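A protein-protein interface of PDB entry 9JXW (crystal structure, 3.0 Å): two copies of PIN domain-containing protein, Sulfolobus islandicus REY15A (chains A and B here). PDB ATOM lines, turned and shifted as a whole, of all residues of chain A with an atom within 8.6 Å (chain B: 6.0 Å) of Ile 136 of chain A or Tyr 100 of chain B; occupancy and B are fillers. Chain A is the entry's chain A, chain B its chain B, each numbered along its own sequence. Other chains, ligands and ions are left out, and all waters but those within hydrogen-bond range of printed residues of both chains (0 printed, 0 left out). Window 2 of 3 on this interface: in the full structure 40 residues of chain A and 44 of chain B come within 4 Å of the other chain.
Among the printed residues, pairs that only touch across the chains: Val 134 of chain A with Tyr 99 of chain B (3.6 Å), Val 134 of chain A with Arg 73 of chain B (3.6 Å), Gly 137 of chain A with Tyr 100 of chain B (3.7 Å) and Gly 137 of chain A with Arg 73 of chain B (3.8 Å).
NE of Arg 77 of chain B sits close to O of Tyr 100 of chain B, 3.4 Å away.
The backbone carbonyl oxygen (O) of Ile 106 of chain A lies within hydrogen-bond range of the backbone NH (N) of Val 134 of chain A, 3.1 Å away.
OH of Tyr 100 of chain B sits at hydrogen-bond distance from O of Ile 136 of chain A (2.4 Å).
Ile 136 of chain A touches just one residue of chain B: Tyr 100.
Of chain A, only Ile 136 (2.4 Å) and Gly 137 (3.7 Å) come within 4 Å of Tyr 100 of chain B.
No residue of chain A comes within 4 Å of Ser 101 of chain B.
Of the printed residues of chain B, Gly 137 of chain A touches Arg 73 and Tyr 100.
Of the printed residues of chain A, Arg 73 of chain B touches Val 134 (3.6 Å) and Gly 137 (3.8 Å).
Printed residues of chain B within 4 Å of Val 134 of chain A: Arg 73 and Tyr 99.
Printed residues of chain A within 4 Å of Tyr 99 of chain B: Val 134.
The nearest printed residue of chain A that does not touch Tyr 99 of chain B is Ile 106 of chain A (4.7 Å).
No position is printed for both chains.
Of the 5 pairs that touch across the chains among the printed residues, none has its exchanged pair printed and touching as well.
Hydrophobic or aromatic side chains of chain A that line the printed part of chain B: Val 134.
Among the printed residues, 5 pairs touch across the chains.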
ATOM      1  N   GLU A 104       6.238  10.315  29.686  1.00  0.00           N
ATOM      2  CA  GLU A 104       7.343  11.261  29.566  1.00  0.00           C
ATOM      3  C   GLU A 104       8.599  10.586  29.028  1.00  0.00           C
ATOM      4  O   GLU A 104       9.314  11.165  28.202  1.00  0.00           O
ATOM      5  CB  GLU A 104       7.619  11.913  30.919  1.00  0.00           C
ATOM      6  CG  GLU A 104       6.461  12.738  31.453  1.00  0.00           C
ATOM      7  CD  GLU A 104       6.746  13.322  32.819  1.00  0.00           C
ATOM      8  OE1 GLU A 104       7.819  13.019  33.385  1.00  0.00           O
ATOM      9  OE2 GLU A 104       5.897  14.081  33.331  1.00  0.00           O
ATOM     10  N   GLU A 105       8.888   9.369  29.485  1.00  0.00           N
ATOM     11  CA  GLU A 105      10.045   8.621  29.019  1.00  0.00           C
ATOM     12  C   GLU A 105       9.619   7.210  28.640  1.00  0.00           C
ATOM     13  O   GLU A 105       8.836   6.576  29.355  1.00  0.00           O
ATOM     14  CB  GLU A 105      11.147   8.582  30.085  1.00  0.00           C
ATOM     15  CG  GLU A 105      12.421   7.884  29.639  1.00  0.00           C
ATOM     16  CD  GLU A 105      13.506   7.925  30.694  1.00  0.00           C
ATOM     17  OE1 GLU A 105      13.295   8.564  31.747  1.00  0.00           O
ATOM     18  OE2 GLU A 105      14.573   7.313  30.473  1.00  0.00           O
ATOM     19  N   ILE A 106      10.129   6.725  27.511  1.00  0.00           N
ATOM     20  CA  ILE A 106       9.871   5.370  27.038  1.00  0.00           C
ATOM     21  C   ILE A 106      11.206   4.674  26.819  1.00  0.00           C
ATOM     22  O   ILE A 106      12.089   5.212  26.140  1.00  0.00           O
ATOM     23  CB  ILE A 106       9.029   5.360  25.748  1.00  0.00           C
ATOM     24  CG1 ILE A 106       7.638   5.937  26.011  1.00  0.00           C
ATOM     25  CG2 ILE A 106       8.919   3.951  25.190  1.00  0.00           C
ATOM     26  CD1 ILE A 106       6.729   5.900  24.807  1.00  0.00           C
ATOM     27  N   ARG A 107      11.351   3.485  27.396  1.00  0.00           N
ATOM     28  CA  ARG A 107      12.586   2.722  27.323  1.00  0.00           C
ATOM     29  C   ARG A 107      12.279   1.265  26.996  1.00  0.00           C
ATOM     30  O   ARG A 107      11.154   0.791  27.168  1.00  0.00           O
ATOM     31  CB  ARG A 107      13.392   2.836  28.625  1.00  0.00           C
ATOM     32  CG  ARG A 107      12.593   2.582  29.888  1.00  0.00           C
ATOM     33  CD  ARG A 107      13.458   2.770  31.124  1.00  0.00           C
ATOM     34  NE  ARG A 107      13.810   4.162  31.381  1.00  0.00           N
ATOM     35  CZ  ARG A 107      14.460   4.579  32.460  1.00  0.00           C
ATOM     36  NH1 ARG A 107      14.837   3.736  33.408  1.00  0.00           N
ATOM     37  NH2 ARG A 107      14.748   5.870  32.587  1.00  0.00           N
ATOM     38  N   ILE A 132      17.534   0.649  27.294  1.00  0.00           N
ATOM     39  CA  ILE A 132      17.805   1.750  26.378  1.00  0.00           C
ATOM     40  C   ILE A 132      16.630   2.714  26.397  1.00  0.00           C
ATOM     41  O   ILE A 132      15.481   2.300  26.208  1.00  0.00           O
ATOM     42  CB  ILE A 132      18.048   1.238  24.948  1.00  0.00           C
ATOM     43  CG1 ILE A 132      19.060   0.098  24.967  1.00  0.00           C
ATOM     44  CG2 ILE A 132      18.509   2.367  24.039  1.00  0.00           C
ATOM     45  CD1 ILE A 132      18.963  -0.778  23.772  1.00  0.00           C
ATOM     46  N   ASN A 133      16.918   3.997  26.604  1.00  0.00           N
ATOM     47  CA  ASN A 133      15.912   5.042  26.424  1.00  0.00           C
ATOM     48  C   ASN A 133      15.706   5.234  24.926  1.00  0.00           C
ATOM     49  O   ASN A 133      16.509   5.887  24.256  1.00  0.00           O
ATOM     50  CB  ASN A 133      16.361   6.333  27.099  1.00  0.00           C
ATOM     51  CG  ASN A 133      15.258   7.377  27.165  1.00  0.00           C
ATOM     52  OD1 ASN A 133      14.288   7.327  26.410  1.00  0.00           O
ATOM     53  ND2 ASN A 133      15.410   8.335  28.072  1.00  0.00           N
ATOM     54  N   VAL A 134      14.621   4.666  24.393  1.00  0.00           N
ATOM     55  CA  VAL A 134      14.396   4.670  22.950  1.00  0.00           C
ATOM     56  C   VAL A 134      14.140   6.064  22.395  1.00  0.00           C
ATOM     57  O   VAL A 134      14.241   6.265  21.178  1.00  0.00           O
ATOM     58  CB  VAL A 134      13.237   3.728  22.584  1.00  0.00           C
ATOM     59  CG1 VAL A 134      13.444   2.375  23.229  1.00  0.00           C
ATOM     60  CG2 VAL A 134      11.908   4.328  23.009  1.00  0.00           C
ATOM     61  N   ARG A 135      13.812   7.037  23.249  1.00  0.00           N
ATOM     62  CA  ARG A 135      13.564   8.386  22.753  1.00  0.00           C
ATOM     63  C   ARG A 135      14.826   8.987  22.151  1.00  0.00           C
ATOM     64  O   ARG A 135      14.773   9.632  21.096  1.00  0.00           O
ATOM     65  CB  ARG A 135      13.037   9.275  23.877  1.00  0.00           C
ATOM     66  CG  ARG A 135      11.739   8.806  24.480  1.00  0.00           C
ATOM     67  CD  ARG A 135      11.295   9.758  25.568  1.00  0.00           C
ATOM     68  NE  ARG A 135       9.906   9.532  25.941  1.00  0.00           N
ATOM     69  CZ  ARG A 135       8.872  10.061  25.304  1.00  0.00           C
ATOM     70  NH1 ARG A 135       9.036  10.855  24.259  1.00  0.00           N
ATOM     71  NH2 ARG A 135       7.640   9.785  25.726  1.00  0.00           N
ATOM     72  N   ILE A 136      15.967   8.797  22.810  1.00  0.00           N
ATOM     73  CA  ILE A 136      17.233   9.328  22.316  1.00  0.00           C
ATOM     74  C   ILE A 136      18.287   8.245  22.113  1.00  0.00           C
ATOM     75  O   ILE A 136      19.362   8.542  21.564  1.00  0.00           O
ATOM     76  CB  ILE A 136      17.772  10.468  23.211  1.00  0.00           C
ATOM     77  CG1 ILE A 136      18.900  10.004  24.121  1.00  0.00           C
ATOM     78  CG2 ILE A 136      16.655  11.070  24.040  1.00  0.00           C
ATOM     79  CD1 ILE A 136      19.456  11.137  24.955  1.00  0.00           C
ATOM     80  N   GLY A 137      18.014   7.005  22.507  1.00  0.00           N
ATOM     81  CA  GLY A 137      18.864   5.873  22.159  1.00  0.00           C
ATOM     82  C   GLY A 137      20.198   5.707  22.862  1.00  0.00           C
ATOM     83  O   GLY A 137      21.184   5.316  22.220  1.00  0.00           O
ATOM     84  N   ASP A 138      20.257   5.972  24.164  1.00  0.00           N
ATOM     85  CA  ASP A 138      21.426   5.652  24.971  1.00  0.00           C
ATOM     86  C   ASP A 138      21.082   4.574  25.994  1.00  0.00           C
ATOM     87  O   ASP A 138      19.919   4.211  26.196  1.00  0.00           O
ATOM     88  CB  ASP A 138      22.006   6.898  25.653  1.00  0.00           C
ATOM     89  CG  ASP A 138      21.042   7.551  26.611  1.00  0.00           C
ATOM     90  OD1 ASP A 138      20.640   6.920  27.612  1.00  0.00           O
ATOM     91  OD2 ASP A 138      20.699   8.719  26.365  1.00  0.00           O
ATOM     92  N   GLU A 139      22.125   4.078  26.658  1.00  0.00           N
ATOM     93  CA  GLU A 139      22.012   2.979  27.611  1.00  0.00           C
ATOM     94  C   GLU A 139      21.867   3.525  29.028  1.00  0.00           C
ATOM     95  O   GLU A 139      22.760   4.219  29.523  1.00  0.00           O
ATOM     96  CB  GLU A 139      23.238   2.071  27.521  1.00  0.00           C
ATOM     97  CG  GLU A 139      23.539   1.594  26.115  1.00  0.00           C
ATOM     98  CD  GLU A 139      24.694   0.625  26.074  1.00  0.00           C
ATOM     99  OE1 GLU A 139      25.412   0.516  27.090  1.00  0.00           O
ATOM    100  OE2 GLU A 139      24.893  -0.017  25.024  1.00  0.00           O
ATOM    101  N   ILE A 140      20.738   3.231  29.661  1.00  0.00           N
ATOM    102  CA  ILE A 140      20.513   3.652  31.048  1.00  0.00           C
ATOM    103  C   ILE A 140      21.371   2.796  31.970  1.00  0.00           C
ATOM    104  O   ILE A 140      21.291   1.553  31.912  1.00  0.00           O
ATOM    105  CB  ILE A 140      19.031   3.524  31.401  1.00  0.00           C
ATOM    106  CG1 ILE A 140      18.158   4.187  30.340  1.00  0.00           C
ATOM    107  CG2 ILE A 140      18.752   4.128  32.768  1.00  0.00           C
ATOM    108  CD1 ILE A 140      18.274   5.697  30.292  1.00  0.00           C
ATOM    109  N   TRP B  72      22.186   0.318  14.577  1.00  0.00           N
ATOM    110  CA  TRP B  72      20.935   0.519  13.853  1.00  0.00           C
ATOM    111  C   TRP B  72      20.438   1.960  13.909  1.00  0.00           C
ATOM    112  O   TRP B  72      19.614   2.343  13.072  1.00  0.00           O
ATOM    113  CB  TRP B  72      19.851  -0.420  14.389  1.00  0.00           C
ATOM    114  CG  TRP B  72      19.892  -1.800  13.793  1.00  0.00           C
ATOM    115  CD1 TRP B  72      20.797  -2.785  14.060  1.00  0.00           C
ATOM    116  CD2 TRP B  72      18.987  -2.340  12.822  1.00  0.00           C
ATOM    117  NE1 TRP B  72      20.510  -3.906  13.319  1.00  0.00           N
ATOM    118  CE2 TRP B  72      19.403  -3.658  12.550  1.00  0.00           C
ATOM    119  CE3 TRP B  72      17.865  -1.837  12.158  1.00  0.00           C
ATOM    120  CZ2 TRP B  72      18.736  -4.479  11.642  1.00  0.00           C
ATOM    121  CZ3 TRP B  72      17.206  -2.652  11.258  1.00  0.00           C
ATOM    122  CH2 TRP B  72      17.643  -3.959  11.007  1.00  0.00           C
ATOM    123  N   ARG B  73      20.909   2.769  14.863  1.00  0.00           N
ATOM    124  CA  ARG B  73      20.514   4.176  14.891  1.00  0.00           C
ATOM    125  C   ARG B  73      21.031   4.919  13.665  1.00  0.00           C
ATOM    126  O   ARG B  73      20.339   5.787  13.119  1.00  0.00           O
ATOM    127  CB  ARG B  73      21.005   4.856  16.172  1.00  0.00           C
ATOM    128  CG  ARG B  73      20.031   4.865  17.356  1.00  0.00           C
ATOM    129  CD  ARG B  73      19.445   3.516  17.714  1.00  0.00           C
ATOM    130  NE  ARG B  73      18.580   3.628  18.883  1.00  0.00           N
ATOM    131  CZ  ARG B  73      17.259   3.728  18.834  1.00  0.00           C
ATOM    132  NH1 ARG B  73      16.605   3.713  17.684  1.00  0.00           N
ATOM    133  NH2 ARG B  73      16.575   3.854  19.968  1.00  0.00           N
ATOM    134  N   GLU B  74      22.240   4.591  13.215  1.00  0.00           N
ATOM    135  CA  GLU B  74      22.892   5.363  12.165  1.00  0.00           C
ATOM    136  C   GLU B  74      22.621   4.794  10.776  1.00  0.00           C
ATOM    137  O   GLU B  74      22.277   5.544   9.858  1.00  0.00           O
ATOM    138  CB  GLU B  74      24.400   5.433  12.437  1.00  0.00           C
ATOM    139  CG  GLU B  74      25.138   6.495  11.635  1.00  0.00           C
ATOM    140  CD  GLU B  74      25.551   6.018  10.259  1.00  0.00           C
ATOM    141  OE1 GLU B  74      25.720   4.793  10.080  1.00  0.00           O
ATOM    142  OE2 GLU B  74      25.701   6.867   9.356  1.00  0.00           O
ATOM    143  N   ILE B  76      20.243   2.955   9.548  1.00  0.00           N
ATOM    144  CA  ILE B  76      18.877   2.843   9.041  1.00  0.00           C
ATOM    145  C   ILE B  76      18.380   4.146   8.433  1.00  0.00           C
ATOM    146  O   ILE B  76      17.341   4.148   7.755  1.00  0.00           O
ATOM    147  CB  ILE B  76      17.922   2.366  10.156  1.00  0.00           C
ATOM    148  CG1 ILE B  76      16.678   1.702   9.560  1.00  0.00           C
ATOM    149  CG2 ILE B  76      17.518   3.519  11.048  1.00  0.00           C
ATOM    150  CD1 ILE B  76      16.950   0.362   8.924  1.00  0.00           C
ATOM    151  N   ARG B  77      19.089   5.255   8.644  1.00  0.00           N
ATOM    152  CA  ARG B  77      18.750   6.528   8.023  1.00  0.00           C
ATOM    153  C   ARG B  77      19.424   6.729   6.672  1.00  0.00           C
ATOM    154  O   ARG B  77      19.098   7.696   5.973  1.00  0.00           O
ATOM    155  CB  ARG B  77      19.122   7.688   8.954  1.00  0.00           C
ATOM    156  CG  ARG B  77      17.947   8.569   9.341  1.00  0.00           C
ATOM    157  CD  ARG B  77      18.307   9.525  10.468  1.00  0.00           C
ATOM    158  NE  ARG B  77      17.143   9.880  11.271  1.00  0.00           N
ATOM    159  CZ  ARG B  77      17.171  10.691  12.320  1.00  0.00           C
ATOM    160  NH1 ARG B  77      18.294  11.265  12.719  1.00  0.00           N
ATOM    161  NH2 ARG B  77      16.045  10.929  12.988  1.00  0.00           N
ATOM    162  N   SER B  96      13.677  -0.008  15.963  1.00  0.00           N
ATOM    163  CA  SER B  96      14.744   0.774  15.350  1.00  0.00           C
ATOM    164  C   SER B  96      14.381   1.300  13.968  1.00  0.00           C
ATOM    165  O   SER B  96      15.111   2.140  13.434  1.00  0.00           O
ATOM    166  CB  SER B  96      16.023  -0.059  15.260  1.00  0.00           C
ATOM    167  OG  SER B  96      16.478  -0.432  16.548  1.00  0.00           O
ATOM    168  N   ALA B  97      13.289   0.822  13.372  1.00  0.00           N
ATOM    169  CA  ALA B  97      12.819   1.369  12.108  1.00  0.00           C
ATOM    170  C   ALA B  97      11.828   2.509  12.297  1.00  0.00           C
ATOM    171  O   ALA B  97      11.755   3.404  11.449  1.00  0.00           O
ATOM    172  CB  ALA B  97      12.184   0.268  11.255  1.00  0.00           C
ATOM    173  N   THR B  98      11.049   2.489  13.381  1.00  0.00           N
ATOM    174  CA  THR B  98      10.189   3.629  13.684  1.00  0.00           C
ATOM    175  C   THR B  98      11.016   4.851  14.068  1.00  0.00           C
ATOM    176  O   THR B  98      10.722   5.971  13.635  1.00  0.00           O
ATOM    177  CB  THR B  98       9.205   3.271  14.798  1.00  0.00           C
ATOM    178  OG1 THR B  98       9.924   2.983  16.003  1.00  0.00           O
ATOM    179  CG2 THR B  98       8.369   2.061  14.404  1.00  0.00           C
ATOM    180  N   TYR B  99      12.049   4.655  14.882  1.00  0.00           N
ATOM    181  CA  TYR B  99      12.942   5.732  15.283  1.00  0.00           C
ATOM    182  C   TYR B  99      14.139   5.806  14.340  1.00  0.00           C
ATOM    183  O   TYR B  99      14.539   4.807  13.737  1.00  0.00           O
ATOM    184  CB  TYR B  99      13.438   5.513  16.714  1.00  0.00           C
ATOM    185  CG  TYR B  99      12.346   5.397  17.755  1.00  0.00           C
ATOM    186  CD1 TYR B  99      11.807   6.523  18.360  1.00  0.00           C
ATOM    187  CD2 TYR B  99      11.865   4.153  18.144  1.00  0.00           C
ATOM    188  CE1 TYR B  99      10.813   6.415  19.317  1.00  0.00           C
ATOM    189  CE2 TYR B  99      10.872   4.034  19.099  1.00  0.00           C
ATOM    190  CZ  TYR B  99      10.349   5.168  19.680  1.00  0.00           C
ATOM    191  OH  TYR B  99       9.361   5.053  20.631  1.00  0.00           O
ATOM    192  N   TYR B 100      14.699   7.012  14.210  1.00  0.00           N
ATOM    193  CA  TYR B 100      15.953   7.237  13.483  1.00  0.00           C
ATOM    194  C   TYR B 100      15.872   6.827  12.014  1.00  0.00           C
ATOM    195  O   TYR B 100      16.892   6.505  11.404  1.00  0.00           O
ATOM    196  CB  TYR B 100      17.120   6.495  14.144  1.00  0.00           C
ATOM    197  CG  TYR B 100      17.556   7.023  15.488  1.00  0.00           C
ATOM    198  CD1 TYR B 100      16.892   6.656  16.650  1.00  0.00           C
ATOM    199  CD2 TYR B 100      18.654   7.865  15.599  1.00  0.00           C
ATOM    200  CE1 TYR B 100      17.298   7.127  17.882  1.00  0.00           C
ATOM    201  CE2 TYR B 100      19.067   8.341  16.825  1.00  0.00           C
ATOM    202  CZ  TYR B 100      18.389   7.967  17.963  1.00  0.00           C
ATOM    203  OH  TYR B 100      18.800   8.446  19.184  1.00  0.00           O
ATOM    204  N   SER B 101      14.686   6.850  11.414  1.00  0.00           N
ATOM    205  CA  SER B 101      14.539   6.441  10.023  1.00  0.00           C
ATOM    206  C   SER B 101      13.789   7.495   9.227  1.00  0.00           C
ATOM    207  O   SER B 101      12.863   8.133   9.735  1.00  0.00           O
ATOM    208  CB  SER B 101      13.813   5.098   9.906  1.00  0.00           C
ATOM    209  OG  SER B 101      12.465   5.209  10.326  1.00  0.00           O
ATOM    210  N   ARG B 102      14.202   7.668   7.972  1.00  0.00           N
ATOM    211  CA  ARG B 102      13.601   8.636   7.069  1.00  0.00           C
ATOM    212  C   ARG B 102      12.463   8.038   6.251  1.00  0.00           C
ATOM    213  O   ARG B 102      12.142   8.561   5.177  1.00  0.00           O
ATOM    214  CB  ARG B 102      14.670   9.199   6.132  1.00  0.00           C
ATOM    215  CG  ARG B 102      15.768   9.972   6.836  1.00  0.00           C
ATOM    216  CD  ARG B 102      16.841  10.414   5.857  1.00  0.00           C
ATOM    217  NE  ARG B 102      17.916  11.141   6.523  1.00  0.00           N
ATOM    218  CZ  ARG B 102      18.999  11.601   5.912  1.00  0.00           C
ATOM    219  NH1 ARG B 102      19.186  11.429   4.614  1.00  0.00           N
ATOM    220  NH2 ARG B 102      19.915  12.252   6.623  1.00  0.00           N
